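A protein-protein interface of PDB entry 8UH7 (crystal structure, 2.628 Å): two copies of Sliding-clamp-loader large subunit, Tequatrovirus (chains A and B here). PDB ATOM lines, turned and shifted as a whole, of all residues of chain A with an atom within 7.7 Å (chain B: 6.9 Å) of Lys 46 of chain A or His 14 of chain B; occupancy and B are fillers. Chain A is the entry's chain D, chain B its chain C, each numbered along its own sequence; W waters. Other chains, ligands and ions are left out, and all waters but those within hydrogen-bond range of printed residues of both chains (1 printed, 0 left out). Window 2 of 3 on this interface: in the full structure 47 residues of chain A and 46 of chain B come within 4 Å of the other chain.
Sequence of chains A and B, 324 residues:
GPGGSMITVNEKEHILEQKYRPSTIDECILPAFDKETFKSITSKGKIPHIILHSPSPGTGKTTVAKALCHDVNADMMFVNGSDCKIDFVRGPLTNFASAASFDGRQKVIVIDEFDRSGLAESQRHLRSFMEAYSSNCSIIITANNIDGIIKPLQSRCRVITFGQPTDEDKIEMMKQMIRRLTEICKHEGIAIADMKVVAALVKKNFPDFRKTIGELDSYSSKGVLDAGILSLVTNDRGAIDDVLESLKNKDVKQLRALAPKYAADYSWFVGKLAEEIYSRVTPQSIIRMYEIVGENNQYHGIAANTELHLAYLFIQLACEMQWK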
ATOM      1  N   SER A  40       5.100   5.389  15.954  1.00  0.00           N
ATOM      2  CA  SER A  40       4.228   4.323  15.472  1.00  0.00           C
ATOM      3  C   SER A  40       4.179   3.167  16.460  1.00  0.00           C
ATOM      4  O   SER A  40       3.103   2.624  16.739  1.00  0.00           O
ATOM      5  CB  SER A  40       4.701   3.837  14.102  1.00  0.00           C
ATOM      6  OG  SER A  40       4.012   2.661  13.715  1.00  0.00           O
ATOM      7  N   ILE A  41       5.336   2.777  17.001  1.00  0.00           N
ATOM      8  CA  ILE A  41       5.380   1.690  17.977  1.00  0.00           C
ATOM      9  C   ILE A  41       4.560   2.046  19.211  1.00  0.00           C
ATOM     10  O   ILE A  41       3.837   1.205  19.757  1.00  0.00           O
ATOM     11  CB  ILE A  41       6.839   1.356  18.348  1.00  0.00           C
ATOM     12  CG1 ILE A  41       7.570   0.745  17.151  1.00  0.00           C
ATOM     13  CG2 ILE A  41       6.888   0.422  19.549  1.00  0.00           C
ATOM     14  CD1 ILE A  41       9.001   0.362  17.444  1.00  0.00           C
ATOM     15  N   THR A  42       4.655   3.298  19.666  1.00  0.00           N
ATOM     16  CA  THR A  42       3.875   3.713  20.828  1.00  0.00           C
ATOM     17  C   THR A  42       2.386   3.774  20.506  1.00  0.00           C
ATOM     18  O   THR A  42       1.550   3.395  21.336  1.00  0.00           O
ATOM     19  CB  THR A  42       4.367   5.065  21.344  1.00  0.00           C
ATOM     20  OG1 THR A  42       4.336   6.026  20.280  1.00  0.00           O
ATOM     21  CG2 THR A  42       5.784   4.948  21.875  1.00  0.00           C
ATOM     22  N   SER A  43       2.033   4.237  19.305  1.00  0.00           N
ATOM     23  CA  SER A  43       0.630   4.324  18.919  1.00  0.00           C
ATOM     24  C   SER A  43      -0.008   2.948  18.788  1.00  0.00           C
ATOM     25  O   SER A  43      -1.205   2.796  19.050  1.00  0.00           O
ATOM     26  CB  SER A  43       0.491   5.095  17.607  1.00  0.00           C
ATOM     27  OG  SER A  43      -0.852   5.091  17.156  1.00  0.00           O
ATOM     28  N   LYS A  44       0.765   1.939  18.374  1.00  0.00           N
ATOM     29  CA  LYS A  44       0.227   0.583  18.337  1.00  0.00           C
ATOM     30  C   LYS A  44       0.023   0.026  19.739  1.00  0.00           C
ATOM     31  O   LYS A  44      -0.865  -0.808  19.948  1.00  0.00           O
ATOM     32  CB  LYS A  44       1.145  -0.334  17.528  1.00  0.00           C
ATOM     33  CG  LYS A  44       1.152  -0.048  16.030  1.00  0.00           C
ATOM     34  CD  LYS A  44       2.182  -0.906  15.311  1.00  0.00           C
ATOM     35  CE  LYS A  44       2.342  -0.479  13.861  1.00  0.00           C
ATOM     36  NZ  LYS A  44       3.529  -1.118  13.228  1.00  0.00           N
ATOM     37  N   GLY A  45       0.825   0.470  20.707  1.00  0.00           N
ATOM     38  CA  GLY A  45       0.679   0.046  22.081  1.00  0.00           C
ATOM     39  C   GLY A  45       1.506  -1.157  22.485  1.00  0.00           C
ATOM     40  O   GLY A  45       1.560  -1.477  23.678  1.00  0.00           O
ATOM     41  N   LYS A  46       2.149  -1.834  21.536  1.00  0.00           N
ATOM     42  CA  LYS A  46       2.973  -3.004  21.815  1.00  0.00           C
ATOM     43  C   LYS A  46       4.382  -2.770  21.288  1.00  0.00           C
ATOM     44  O   LYS A  46       4.559  -2.342  20.143  1.00  0.00           O
ATOM     45  CB  LYS A  46       2.371  -4.262  21.185  1.00  0.00           C
ATOM     46  CG  LYS A  46       1.004  -4.648  21.736  1.00  0.00           C
ATOM     47  CD  LYS A  46       1.082  -4.999  23.214  1.00  0.00           C
ATOM     48  CE  LYS A  46      -0.235  -5.562  23.729  1.00  0.00           C
ATOM     49  NZ  LYS A  46      -0.603  -6.836  23.049  1.00  0.00           N
ATOM     50  N   ILE A  47       5.374  -3.055  22.119  1.00  0.00           N
ATOM     51  CA  ILE A  47       6.782  -2.855  21.783  1.00  0.00           C
ATOM     52  C   ILE A  47       7.365  -4.188  21.328  1.00  0.00           C
ATOM     53  O   ILE A  47       7.209  -5.191  22.039  1.00  0.00           O
ATOM     54  CB  ILE A  47       7.573  -2.299  22.981  1.00  0.00           C
ATOM     55  CG1 ILE A  47       7.064  -0.911  23.363  1.00  0.00           C
ATOM     56  CG2 ILE A  47       9.060  -2.248  22.671  1.00  0.00           C
ATOM     57  CD1 ILE A  47       7.855  -0.265  24.480  1.00  0.00           C
ATOM     58  N   PRO A  48       8.028  -4.249  20.180  1.00  0.00           N
ATOM     59  CA  PRO A  48       8.708  -5.478  19.765  1.00  0.00           C
ATOM     60  C   PRO A  48      10.094  -5.560  20.397  1.00  0.00           C
ATOM     61  O   PRO A  48      10.497  -4.710  21.187  1.00  0.00           O
ATOM     62  CB  PRO A  48       8.796  -5.320  18.249  1.00  0.00           C
ATOM     63  CG  PRO A  48       8.945  -3.846  18.063  1.00  0.00           C
ATOM     64  CD  PRO A  48       8.115  -3.200  19.150  1.00  0.00           C
ATOM     65  N   HIS A  49      10.824  -6.611  20.035  1.00  0.00           N
ATOM     66  CA  HIS A  49      12.227  -6.712  20.418  1.00  0.00           C
ATOM     67  C   HIS A  49      13.037  -5.710  19.604  1.00  0.00           C
ATOM     68  O   HIS A  49      12.998  -5.732  18.370  1.00  0.00           O
ATOM     69  CB  HIS A  49      12.741  -8.128  20.186  1.00  0.00           C
ATOM     70  CG  HIS A  49      11.929  -9.187  20.864  1.00  0.00           C
ATOM     71  ND1 HIS A  49      11.781  -9.251  22.233  1.00  0.00           N
ATOM     72  CD2 HIS A  49      11.234 -10.234  20.362  1.00  0.00           C
ATOM     73  CE1 HIS A  49      11.024 -10.288  22.544  1.00  0.00           C
ATOM     74  NE2 HIS A  49      10.679 -10.902  21.427  1.00  0.00           N
ATOM     75  N   ILE A  50      13.763  -4.827  20.286  1.00  0.00           N
ATOM     76  CA  ILE A  50      14.499  -3.762  19.616  1.00  0.00           C
ATOM     77  C   ILE A  50      15.962  -3.828  20.022  1.00  0.00           C
ATOM     78  O   ILE A  50      16.297  -4.242  21.135  1.00  0.00           O
ATOM     79  CB  ILE A  50      13.917  -2.366  19.934  1.00  0.00           C
ATOM     80  CG1 ILE A  50      12.390  -2.398  19.942  1.00  0.00           C
ATOM     81  CG2 ILE A  50      14.375  -1.351  18.909  1.00  0.00           C
ATOM     82  CD1 ILE A  50      11.762  -1.041  20.162  1.00  0.00           C
ATOM     83  N   LEU A  68      10.322   4.833  25.416  1.00  0.00           N
ATOM     84  CA  LEU A  68       9.365   3.880  24.867  1.00  0.00           C
ATOM     85  C   LEU A  68       8.604   3.182  25.983  1.00  0.00           C
ATOM     86  O   LEU A  68       7.369   3.099  25.953  1.00  0.00           O
ATOM     87  CB  LEU A  68      10.084   2.855  23.988  1.00  0.00           C
ATOM     88  CG  LEU A  68      10.282   3.190  22.511  1.00  0.00           C
ATOM     89  CD1 LEU A  68      11.244   2.205  21.879  1.00  0.00           C
ATOM     90  CD2 LEU A  68       8.951   3.162  21.792  1.00  0.00           C
ATOM     91  N   VAL A  72       4.529   3.766  26.376  1.00  0.00           N
ATOM     92  CA  VAL A  72       3.656   2.597  26.294  1.00  0.00           C
ATOM     93  C   VAL A  72       3.075   2.225  27.650  1.00  0.00           C
ATOM     94  O   VAL A  72       2.121   1.438  27.715  1.00  0.00           O
ATOM     95  CB  VAL A  72       4.454   1.454  25.635  1.00  0.00           C
ATOM     96  CG1 VAL A  72       3.637   0.173  25.525  1.00  0.00           C
ATOM     97  CG2 VAL A  72       4.915   1.887  24.253  1.00  0.00           C
ATOM     98  N   GLY A 104      -2.986  -5.386  32.371  1.00  0.00           N
ATOM     99  CA  GLY A 104      -2.894  -5.224  30.935  1.00  0.00           C
ATOM    100  C   GLY A 104      -1.651  -4.522  30.439  1.00  0.00           C
ATOM    101  O   GLY A 104      -1.570  -4.213  29.245  1.00  0.00           O
ATOM    102  N   ARG A 105      -0.682  -4.257  31.310  1.00  0.00           N
ATOM    103  CA  ARG A 105       0.554  -3.612  30.894  1.00  0.00           C
ATOM    104  C   ARG A 105       1.504  -4.625  30.271  1.00  0.00           C
ATOM    105  O   ARG A 105       1.558  -5.788  30.680  1.00  0.00           O
ATOM    106  CB  ARG A 105       1.227  -2.930  32.085  1.00  0.00           C
ATOM    107  CG  ARG A 105       0.399  -1.832  32.723  1.00  0.00           C
ATOM    108  CD  ARG A 105       0.939  -1.475  34.093  1.00  0.00           C
ATOM    109  NE  ARG A 105       2.296  -0.943  34.031  1.00  0.00           N
ATOM    110  CZ  ARG A 105       3.099  -0.835  35.084  1.00  0.00           C
ATOM    111  NH1 ARG A 105       2.681  -1.231  36.279  1.00  0.00           N
ATOM    112  NH2 ARG A 105       4.320  -0.337  34.943  1.00  0.00           N
ATOM    113  N   GLN A 106       2.255  -4.174  29.272  1.00  0.00           N
ATOM    114  CA  GLN A 106       3.253  -5.023  28.640  1.00  0.00           C
ATOM    115  C   GLN A 106       4.521  -5.054  29.480  1.00  0.00           C
ATOM    116  O   GLN A 106       4.955  -4.030  30.012  1.00  0.00           O
ATOM    117  CB  GLN A 106       3.574  -4.520  27.233  1.00  0.00           C
ATOM    118  CG  GLN A 106       4.606  -5.360  26.504  1.00  0.00           C
ATOM    119  CD  GLN A 106       4.883  -4.852  25.108  1.00  0.00           C
ATOM    120  OE1 GLN A 106       4.561  -3.711  24.777  1.00  0.00           O
ATOM    121  NE2 GLN A 106       5.479  -5.700  24.278  1.00  0.00           N
ATOM    122  N   LYS A 107       5.110  -6.238  29.605  1.00  0.00           N
ATOM    123  CA  LYS A 107       6.374  -6.387  30.310  1.00  0.00           C
ATOM    124  C   LYS A 107       7.522  -6.221  29.324  1.00  0.00           C
ATOM    125  O   LYS A 107       7.553  -6.881  28.282  1.00  0.00           O
ATOM    126  CB  LYS A 107       6.448  -7.745  31.005  1.00  0.00           C
ATOM    127  CG  LYS A 107       5.520  -7.860  32.204  1.00  0.00           C
ATOM    128  CD  LYS A 107       5.658  -9.201  32.899  1.00  0.00           C
ATOM    129  CE  LYS A 107       5.039  -9.154  34.286  1.00  0.00           C
ATOM    130  NZ  LYS A 107       5.669  -8.105  35.142  1.00  0.00           N
ATOM    131  N   VAL A 108       8.453  -5.323  29.645  1.00  0.00           N
ATOM    132  CA  VAL A 108       9.605  -5.046  28.795  1.00  0.00           C
ATOM    133  C   VAL A 108      10.864  -5.116  29.645  1.00  0.00           C
ATOM    134  O   VAL A 108      10.924  -4.518  30.725  1.00  0.00           O
ATOM    135  CB  VAL A 108       9.497  -3.675  28.101  1.00  0.00           C
ATOM    136  CG1 VAL A 108      10.774  -3.367  27.339  1.00  0.00           C
ATOM    137  CG2 VAL A 108       8.306  -3.649  27.162  1.00  0.00           C
ATOM    138  N   TYR A 133       8.468 -16.390  25.493  1.00  0.00           N
ATOM    139  CA  TYR A 133       7.738 -15.338  26.187  1.00  0.00           C
ATOM    140  C   TYR A 133       7.452 -14.138  25.291  1.00  0.00           C
ATOM    141  O   TYR A 133       7.308 -13.017  25.787  1.00  0.00           O
ATOM    142  CB  TYR A 133       8.514 -14.895  27.426  1.00  0.00           C
ATOM    143  CG  TYR A 133       8.761 -15.995  28.436  1.00  0.00           C
ATOM    144  CD1 TYR A 133       7.968 -16.113  29.569  1.00  0.00           C
ATOM    145  CD2 TYR A 133       9.790 -16.912  28.260  1.00  0.00           C
ATOM    146  CE1 TYR A 133       8.190 -17.114  30.495  1.00  0.00           C
ATOM    147  CE2 TYR A 133      10.016 -17.918  29.180  1.00  0.00           C
ATOM    148  CZ  TYR A 133       9.214 -18.013  30.296  1.00  0.00           C
ATOM    149  OH  TYR A 133       9.436 -19.011  31.219  1.00  0.00           O
ATOM    150  N   SER A 134       7.364 -14.350  23.976  1.00  0.00           N
ATOM    151  CA  SER A 134       7.167 -13.236  23.055  1.00  0.00           C
ATOM    152  C   SER A 134       5.757 -12.670  23.099  1.00  0.00           C
ATOM    153  O   SER A 134       5.530 -11.582  22.560  1.00  0.00           O
ATOM    154  CB  SER A 134       7.485 -13.671  21.626  1.00  0.00           C
ATOM    155  OG  SER A 134       6.510 -14.581  21.150  1.00  0.00           O
ATOM    156  N   SER A 135       4.810 -13.374  23.716  1.00  0.00           N
ATOM    157  CA  SER A 135       3.433 -12.897  23.727  1.00  0.00           C
ATOM    158  C   SER A 135       3.265 -11.705  24.658  1.00  0.00           C
ATOM    159  O   SER A 135       2.558 -10.746  24.327  1.00  0.00           O
ATOM    160  CB  SER A 135       2.491 -14.031  24.127  1.00  0.00           C
ATOM    161  OG  SER A 135       2.901 -14.623  25.348  1.00  0.00           O
ATOM    162  N   ASN A 136       3.915 -11.737  25.823  1.00  0.00           N
ATOM    163  CA  ASN A 136       3.739 -10.705  26.834  1.00  0.00           C
ATOM    164  C   ASN A 136       5.002  -9.923  27.161  1.00  0.00           C
ATOM    165  O   ASN A 136       4.895  -8.826  27.718  1.00  0.00           O
ATOM    166  CB  ASN A 136       3.196 -11.319  28.135  1.00  0.00           C
ATOM    167  CG  ASN A 136       2.724 -10.271  29.125  1.00  0.00           C
ATOM    168  OD1 ASN A 136       2.319  -9.172  28.738  1.00  0.00           O
ATOM    169  ND2 ASN A 136       2.780 -10.607  30.413  1.00  0.00           N
ATOM    170  N   CYS A 137       6.182 -10.439  26.830  1.00  0.00           N
ATOM    171  CA  CYS A 137       7.441  -9.821  27.220  1.00  0.00           C
ATOM    172  C   CYS A 137       8.283  -9.527  25.988  1.00  0.00           C
ATOM    173  O   CYS A 137       8.449 -10.393  25.123  1.00  0.00           O
ATOM    174  CB  CYS A 137       8.212 -10.721  28.187  1.00  0.00           C
ATOM    175  SG  CYS A 137       9.731  -9.994  28.809  1.00  0.00           S
ATOM    176  N   SER A 138       8.813  -8.308  25.916  1.00  0.00           N
ATOM    177  CA  SER A 138       9.711  -7.887  24.851  1.00  0.00           C
ATOM    178  C   SER A 138      11.002  -7.347  25.451  1.00  0.00           C
ATOM    179  O   SER A 138      11.040  -6.907  26.604  1.00  0.00           O
ATOM    180  CB  SER A 138       9.069  -6.819  23.959  1.00  0.00           C
ATOM    181  OG  SER A 138       7.885  -7.305  23.355  1.00  0.00           O
ATOM    182  N   ARG A 158      14.303  -5.617  15.988  1.00  0.00           N
ATOM    183  CA  ARG A 158      14.323  -4.457  15.104  1.00  0.00           C
ATOM    184  C   ARG A 158      15.602  -3.680  15.382  1.00  0.00           C
ATOM    185  O   ARG A 158      15.752  -3.085  16.452  1.00  0.00           O
ATOM    186  CB  ARG A 158      13.094  -3.582  15.337  1.00  0.00           C
ATOM    187  CG  ARG A 158      11.876  -3.927  14.495  1.00  0.00           C
ATOM    188  CD  ARG A 158      11.377  -5.332  14.760  1.00  0.00           C
ATOM    189  NE  ARG A 158       9.982  -5.499  14.369  1.00  0.00           N
ATOM    190  CZ  ARG A 158       9.371  -6.673  14.290  1.00  0.00           C
ATOM    191  NH1 ARG A 158      10.036  -7.784  14.568  1.00  0.00           N
ATOM    192  NH2 ARG A 158       8.097  -6.740  13.929  1.00  0.00           N
ATOM    193  N   ASN B  10      -0.941 -17.060  14.793  1.00  0.00           N
ATOM    194  CA  ASN B  10      -0.986 -17.159  16.251  1.00  0.00           C
ATOM    195  C   ASN B  10      -1.654 -15.902  16.783  1.00  0.00           C
ATOM    196  O   ASN B  10      -1.024 -14.847  16.894  1.00  0.00           O
ATOM    197  CB  ASN B  10       0.410 -17.326  16.838  1.00  0.00           C
ATOM    198  CG  ASN B  10       1.027 -18.662  16.502  1.00  0.00           C
ATOM    199  OD1 ASN B  10       0.818 -19.200  15.414  1.00  0.00           O
ATOM    200  ND2 ASN B  10       1.792 -19.214  17.439  1.00  0.00           N
ATOM    201  N   GLU B  11      -2.941 -16.010  17.112  1.00  0.00           N
ATOM    202  CA  GLU B  11      -3.685 -14.862  17.611  1.00  0.00           C
ATOM    203  C   GLU B  11      -3.123 -14.333  18.926  1.00  0.00           C
ATOM    204  O   GLU B  11      -3.398 -13.184  19.286  1.00  0.00           O
ATOM    205  CB  GLU B  11      -5.163 -15.233  17.778  1.00  0.00           C
ATOM    206  CG  GLU B  11      -5.418 -16.503  18.595  1.00  0.00           C
ATOM    207  CD  GLU B  11      -5.288 -17.783  17.776  1.00  0.00           C
ATOM    208  OE1 GLU B  11      -5.249 -17.700  16.529  1.00  0.00           O
ATOM    209  OE2 GLU B  11      -5.225 -18.873  18.382  1.00  0.00           O
ATOM    210  N   LYS B  12      -2.335 -15.132  19.640  1.00  0.00           N
ATOM    211  CA  LYS B  12      -1.775 -14.732  20.923  1.00  0.00           C
ATOM    212  C   LYS B  12      -0.487 -13.926  20.792  1.00  0.00           C
ATOM    213  O   LYS B  12       0.035 -13.452  21.806  1.00  0.00           O
ATOM    214  CB  LYS B  12      -1.519 -15.970  21.789  1.00  0.00           C
ATOM    215  CG  LYS B  12      -2.688 -16.943  21.835  1.00  0.00           C
ATOM    216  CD  LYS B  12      -2.350 -18.186  22.644  1.00  0.00           C
ATOM    217  CE  LYS B  12      -3.490 -19.199  22.615  1.00  0.00           C
ATOM    218  NZ  LYS B  12      -3.756 -19.728  21.245  1.00  0.00           N
ATOM    219  N   GLU B  13       0.032 -13.753  19.580  1.00  0.00           N
ATOM    220  CA  GLU B  13       1.296 -13.070  19.345  1.00  0.00           C
ATOM    221  C   GLU B  13       1.058 -11.752  18.623  1.00  0.00           C
ATOM    222  O   GLU B  13       0.193 -11.662  17.747  1.00  0.00           O
ATOM    223  CB  GLU B  13       2.244 -13.942  18.517  1.00  0.00           C
ATOM    224  CG  GLU B  13       2.631 -15.246  19.183  1.00  0.00           C
ATOM    225  CD  GLU B  13       3.629 -15.052  20.306  1.00  0.00           C
ATOM    226  OE1 GLU B  13       4.253 -13.968  20.373  1.00  0.00           O
ATOM    227  OE2 GLU B  13       3.793 -15.986  21.119  1.00  0.00           O
ATOM    228  N   HIS B  14       1.834 -10.733  18.985  1.00  0.00           N
ATOM    229  CA  HIS B  14       1.757  -9.447  18.305  1.00  0.00           C
ATOM    230  C   HIS B  14       2.951  -9.164  17.410  1.00  0.00           C
ATOM    231  O   HIS B  14       2.801  -8.455  16.413  1.00  0.00           O
ATOM    232  CB  HIS B  14       1.613  -8.309  19.322  1.00  0.00           C
ATOM    233  CG  HIS B  14       2.832  -8.086  20.158  1.00  0.00           C
ATOM    234  ND1 HIS B  14       3.809  -7.176  19.818  1.00  0.00           N
ATOM    235  CD2 HIS B  14       3.235  -8.657  21.319  1.00  0.00           C
ATOM    236  CE1 HIS B  14       4.761  -7.193  20.735  1.00  0.00           C
ATOM    237  NE2 HIS B  14       4.437  -8.083  21.656  1.00  0.00           N
ATOM    238  N   ILE B  15       4.126  -9.704  17.736  1.00  0.00           N
ATOM    239  CA  ILE B  15       5.287  -9.566  16.868  1.00  0.00           C
ATOM    240  C   ILE B  15       5.027 -10.311  15.568  1.00  0.00           C
ATOM    241  O   ILE B  15       4.611 -11.476  15.574  1.00  0.00           O
ATOM    242  CB  ILE B  15       6.547 -10.089  17.570  1.00  0.00           C
ATOM    243  CG1 ILE B  15       6.698  -9.432  18.941  1.00  0.00           C
ATOM    244  CG2 ILE B  15       7.772  -9.809  16.727  1.00  0.00           C
ATOM    245  CD1 ILE B  15       7.882  -9.935  19.729  1.00  0.00           C
ATOM    246  N   LEU B  16       5.278  -9.640  14.442  1.00  0.00           N
ATOM    247  CA  LEU B  16       4.860 -10.163  13.144  1.00  0.00           C
ATOM    248  C   LEU B  16       5.448 -11.544  12.874  1.00  0.00           C
ATOM    249  O   LEU B  16       4.723 -12.473  12.503  1.00  0.00           O
ATOM    250  CB  LEU B  16       5.255  -9.187  12.038  1.00  0.00           C
ATOM    251  CG  LEU B  16       4.097  -8.526  11.300  1.00  0.00           C
ATOM    252  CD1 LEU B  16       3.252  -7.725  12.274  1.00  0.00           C
ATOM    253  CD2 LEU B  16       4.631  -7.648  10.184  1.00  0.00           C
ATOM    254  N   GLU B  17       6.764 -11.700  13.049  1.00  0.00           N
ATOM    255  CA  GLU B  17       7.393 -12.982  12.743  1.00  0.00           C
ATOM    256  C   GLU B  17       6.922 -14.098  13.665  1.00  0.00           C
ATOM    257  O   GLU B  17       7.013 -15.271  13.289  1.00  0.00           O
ATOM    258  CB  GLU B  17       8.917 -12.867  12.804  1.00  0.00           C
ATOM    259  CG  GLU B  17       9.462 -12.292  14.093  1.00  0.00           C
ATOM    260  CD  GLU B  17       9.631 -10.788  14.030  1.00  0.00           C
ATOM    261  OE1 GLU B  17       8.849 -10.130  13.312  1.00  0.00           O
ATOM    262  OE2 GLU B  17      10.548 -10.264  14.696  1.00  0.00           O
ATOM    263  N   GLN B  18       6.420 -13.765  14.856  1.00  0.00           N
ATOM    264  CA  GLN B  18       5.826 -14.776  15.723  1.00  0.00           C
ATOM    265  C   GLN B  18       4.370 -15.043  15.371  1.00  0.00           C
ATOM    266  O   GLN B  18       3.889 -16.166  15.550  1.00  0.00           O
ATOM    267  CB  GLN B  18       5.930 -14.352  17.188  1.00  0.00           C
ATOM    268  CG  GLN B  18       7.339 -14.338  17.735  1.00  0.00           C
ATOM    269  CD  GLN B  18       7.861 -15.728  18.033  1.00  0.00           C
ATOM    270  OE1 GLN B  18       7.831 -16.619  17.183  1.00  0.00           O
ATOM    271  NE2 GLN B  18       8.342 -15.923  19.253  1.00  0.00           N
ATOM    272  N   LYS B  19       3.662 -14.026  14.878  1.00  0.00           N
ATOM    273  CA  LYS B  19       2.249 -14.186  14.557  1.00  0.00           C
ATOM    274  C   LYS B  19       2.056 -15.066  13.327  1.00  0.00           C
ATOM    275  O   LYS B  19       1.149 -15.906  13.293  1.00  0.00           O
ATOM    276  CB  LYS B  19       1.613 -12.811  14.347  1.00  0.00           C
ATOM    277  CG  LYS B  19       0.106 -12.819  14.184  1.00  0.00           C
ATOM    278  CD  LYS B  19      -0.436 -11.404  14.100  1.00  0.00           C
ATOM    279  CE  LYS B  19      -1.948 -11.405  13.969  1.00  0.00           C
ATOM    280  NZ  LYS B  19      -2.503 -10.029  13.835  1.00  0.00           N
ATOM    281  N   GLU B 188      -2.694  -7.363   7.469  1.00  0.00           N
ATOM    282  CA  GLU B 188      -2.306  -6.426   8.521  1.00  0.00           C
ATOM    283  C   GLU B 188      -2.762  -5.001   8.263  1.00  0.00           C
ATOM    284  O   GLU B 188      -2.818  -4.205   9.207  1.00  0.00           O
ATOM    285  CB  GLU B 188      -0.785  -6.435   8.700  1.00  0.00           C
ATOM    286  CG  GLU B 188      -0.255  -7.648   9.432  1.00  0.00           C
ATOM    287  CD  GLU B 188      -0.686  -7.675  10.881  1.00  0.00           C
ATOM    288  OE1 GLU B 188      -0.703  -6.598  11.514  1.00  0.00           O
ATOM    289  OE2 GLU B 188      -1.017  -8.769  11.384  1.00  0.00           O
ATOM    290  N   ASP B 217       7.892  -4.931   8.952  1.00  0.00           N
ATOM    291  CA  ASP B 217       7.217  -4.209  10.026  1.00  0.00           C
ATOM    292  C   ASP B 217       7.906  -2.887  10.335  1.00  0.00           C
ATOM    293  O   ASP B 217       7.246  -1.930  10.754  1.00  0.00           O
ATOM    294  CB  ASP B 217       7.154  -5.073  11.284  1.00  0.00           C
ATOM    295  CG  ASP B 217       6.296  -4.454  12.375  1.00  0.00           C
ATOM    296  OD1 ASP B 217       5.398  -3.649  12.045  1.00  0.00           O
ATOM    297  OD2 ASP B 217       6.523  -4.767  13.564  1.00  0.00           O
HETATM  298  O   HOH W   1       5.955  -8.897  23.485  1.00  0.00           O
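The guanidinium group of Arg 158 of chain A is in salt-bridge range of the side-chain carboxylate of Glu 17 of chain B, at 2.5 Å.
OD1 of Asp 217 of chain B lies within salt-bridge range of NZ of Lys 44 of chain A, 3.4 Å away.
NE2 of Gln 18 of chain B is in hydrogen-bond range of OG of Ser 134 of chain A, 3.0 Å away.
The side-chain carboxylate (OD2) of Asp 217 of chain B is in salt-bridge range of the guanidinium group (NH2) of Arg 158 of chain A.
The side-chain carboxylate (OE1) of Glu 13 of chain B is in hydrogen-bond range of the side-chain hydroxyl (OG) of Ser 134 of chain A, at 2.5 Å.
The side-chain carboxylate of Glu 13 of chain B is in hydrogen-bond range of the backbone NH of Ser 135 of chain A (3.4 Å).
The side-chain carboxylate (OE2) of Glu 11 of chain B is in salt-bridge range of the side-chain amino group (NZ) of Lys 12 of chain B (3.3 Å).
The side-chain amide nitrogen of Gln 106 of chain A is in hydrogen-bond range of the side-chain hydroxyl of Ser 138 of chain A, 3.0 Å away.
His 14 of chain B touches Lys 46 of chain A (ND1 to CB, 3.5 Å).
CE1 of His 14 of chain B touches O of Ile 47 of chain A (3.4 Å).
NE2 of Gln 106 of chain A touches NE2 of His 14 of chain B, at 3.7 Å.
His 14 of chain B touches Ser 134 of chain A (NE2 to O, 3.8 Å).
Ser 135 of chain A touches Lys 12 of chain B (CB to O, 3.4 Å).
Lys 46 of chain A touches just one residue of chain B: His 14 (3.5 Å).
His 14 of chain B touches just these residues of chain A: Lys 46, Ile 47, Gln 106, Ser 134, Ser 135 and Ser 138.
Of the printed residues of chain A, Glu 13 of chain B touches Ser 134 (2.5 Å) and Ser 135 (3.4 Å).
Of the printed residues of chain B, Ile 47 of chain A touches His 14 (3.4 Å).
The nearest residue of chain B that does not touch Lys 46 of chain A is Ile 15 of chain B (6.7 Å).
The nearest residue of chain A that does not touch His 14 of chain B is Pro 48 of chain A (4.4 Å).
The nearest printed residue of chain B that does not touch Lys 44 of chain A is Leu 16 of chain B (6.7 Å).
Of the 12 printed residues of chain B, 7 touch a printed residue of chain A.
Printed residues of chain B that touch a printed residue of chain A: Lys 12, Glu 13, His 14, Ile 15, Glu 17, Gln 18 and Asp 217.
Hydrophobic or aromatic side chains of chain B that line the printed part of chain A: His 14 and Ile 15.
Of the 25 printed residues of chain A, 9 touch a printed residue of chain B.
Hydrophobic or aromatic side chains of chain A that line the printed part of chain B: His 49.
Among the printed residues, 15 pairs touch across the chains.
Among the printed residues, Asp or Glu carboxylates within 4 Å of a Lys or Arg side-chain nitrogen of the other chain: Lys 44 of chain A with Asp 217 of chain B (3.4 Å), Arg 158 of chain A with Glu 17 of chain B (2.5 Å) and Arg 158 of chain A with Asp 217 of chain B (2.6 Å).
No position is printed for both chains.
Of the 15 pairs that touch across the chains among the printed residues, none has its exchanged pair printed and touching as well.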
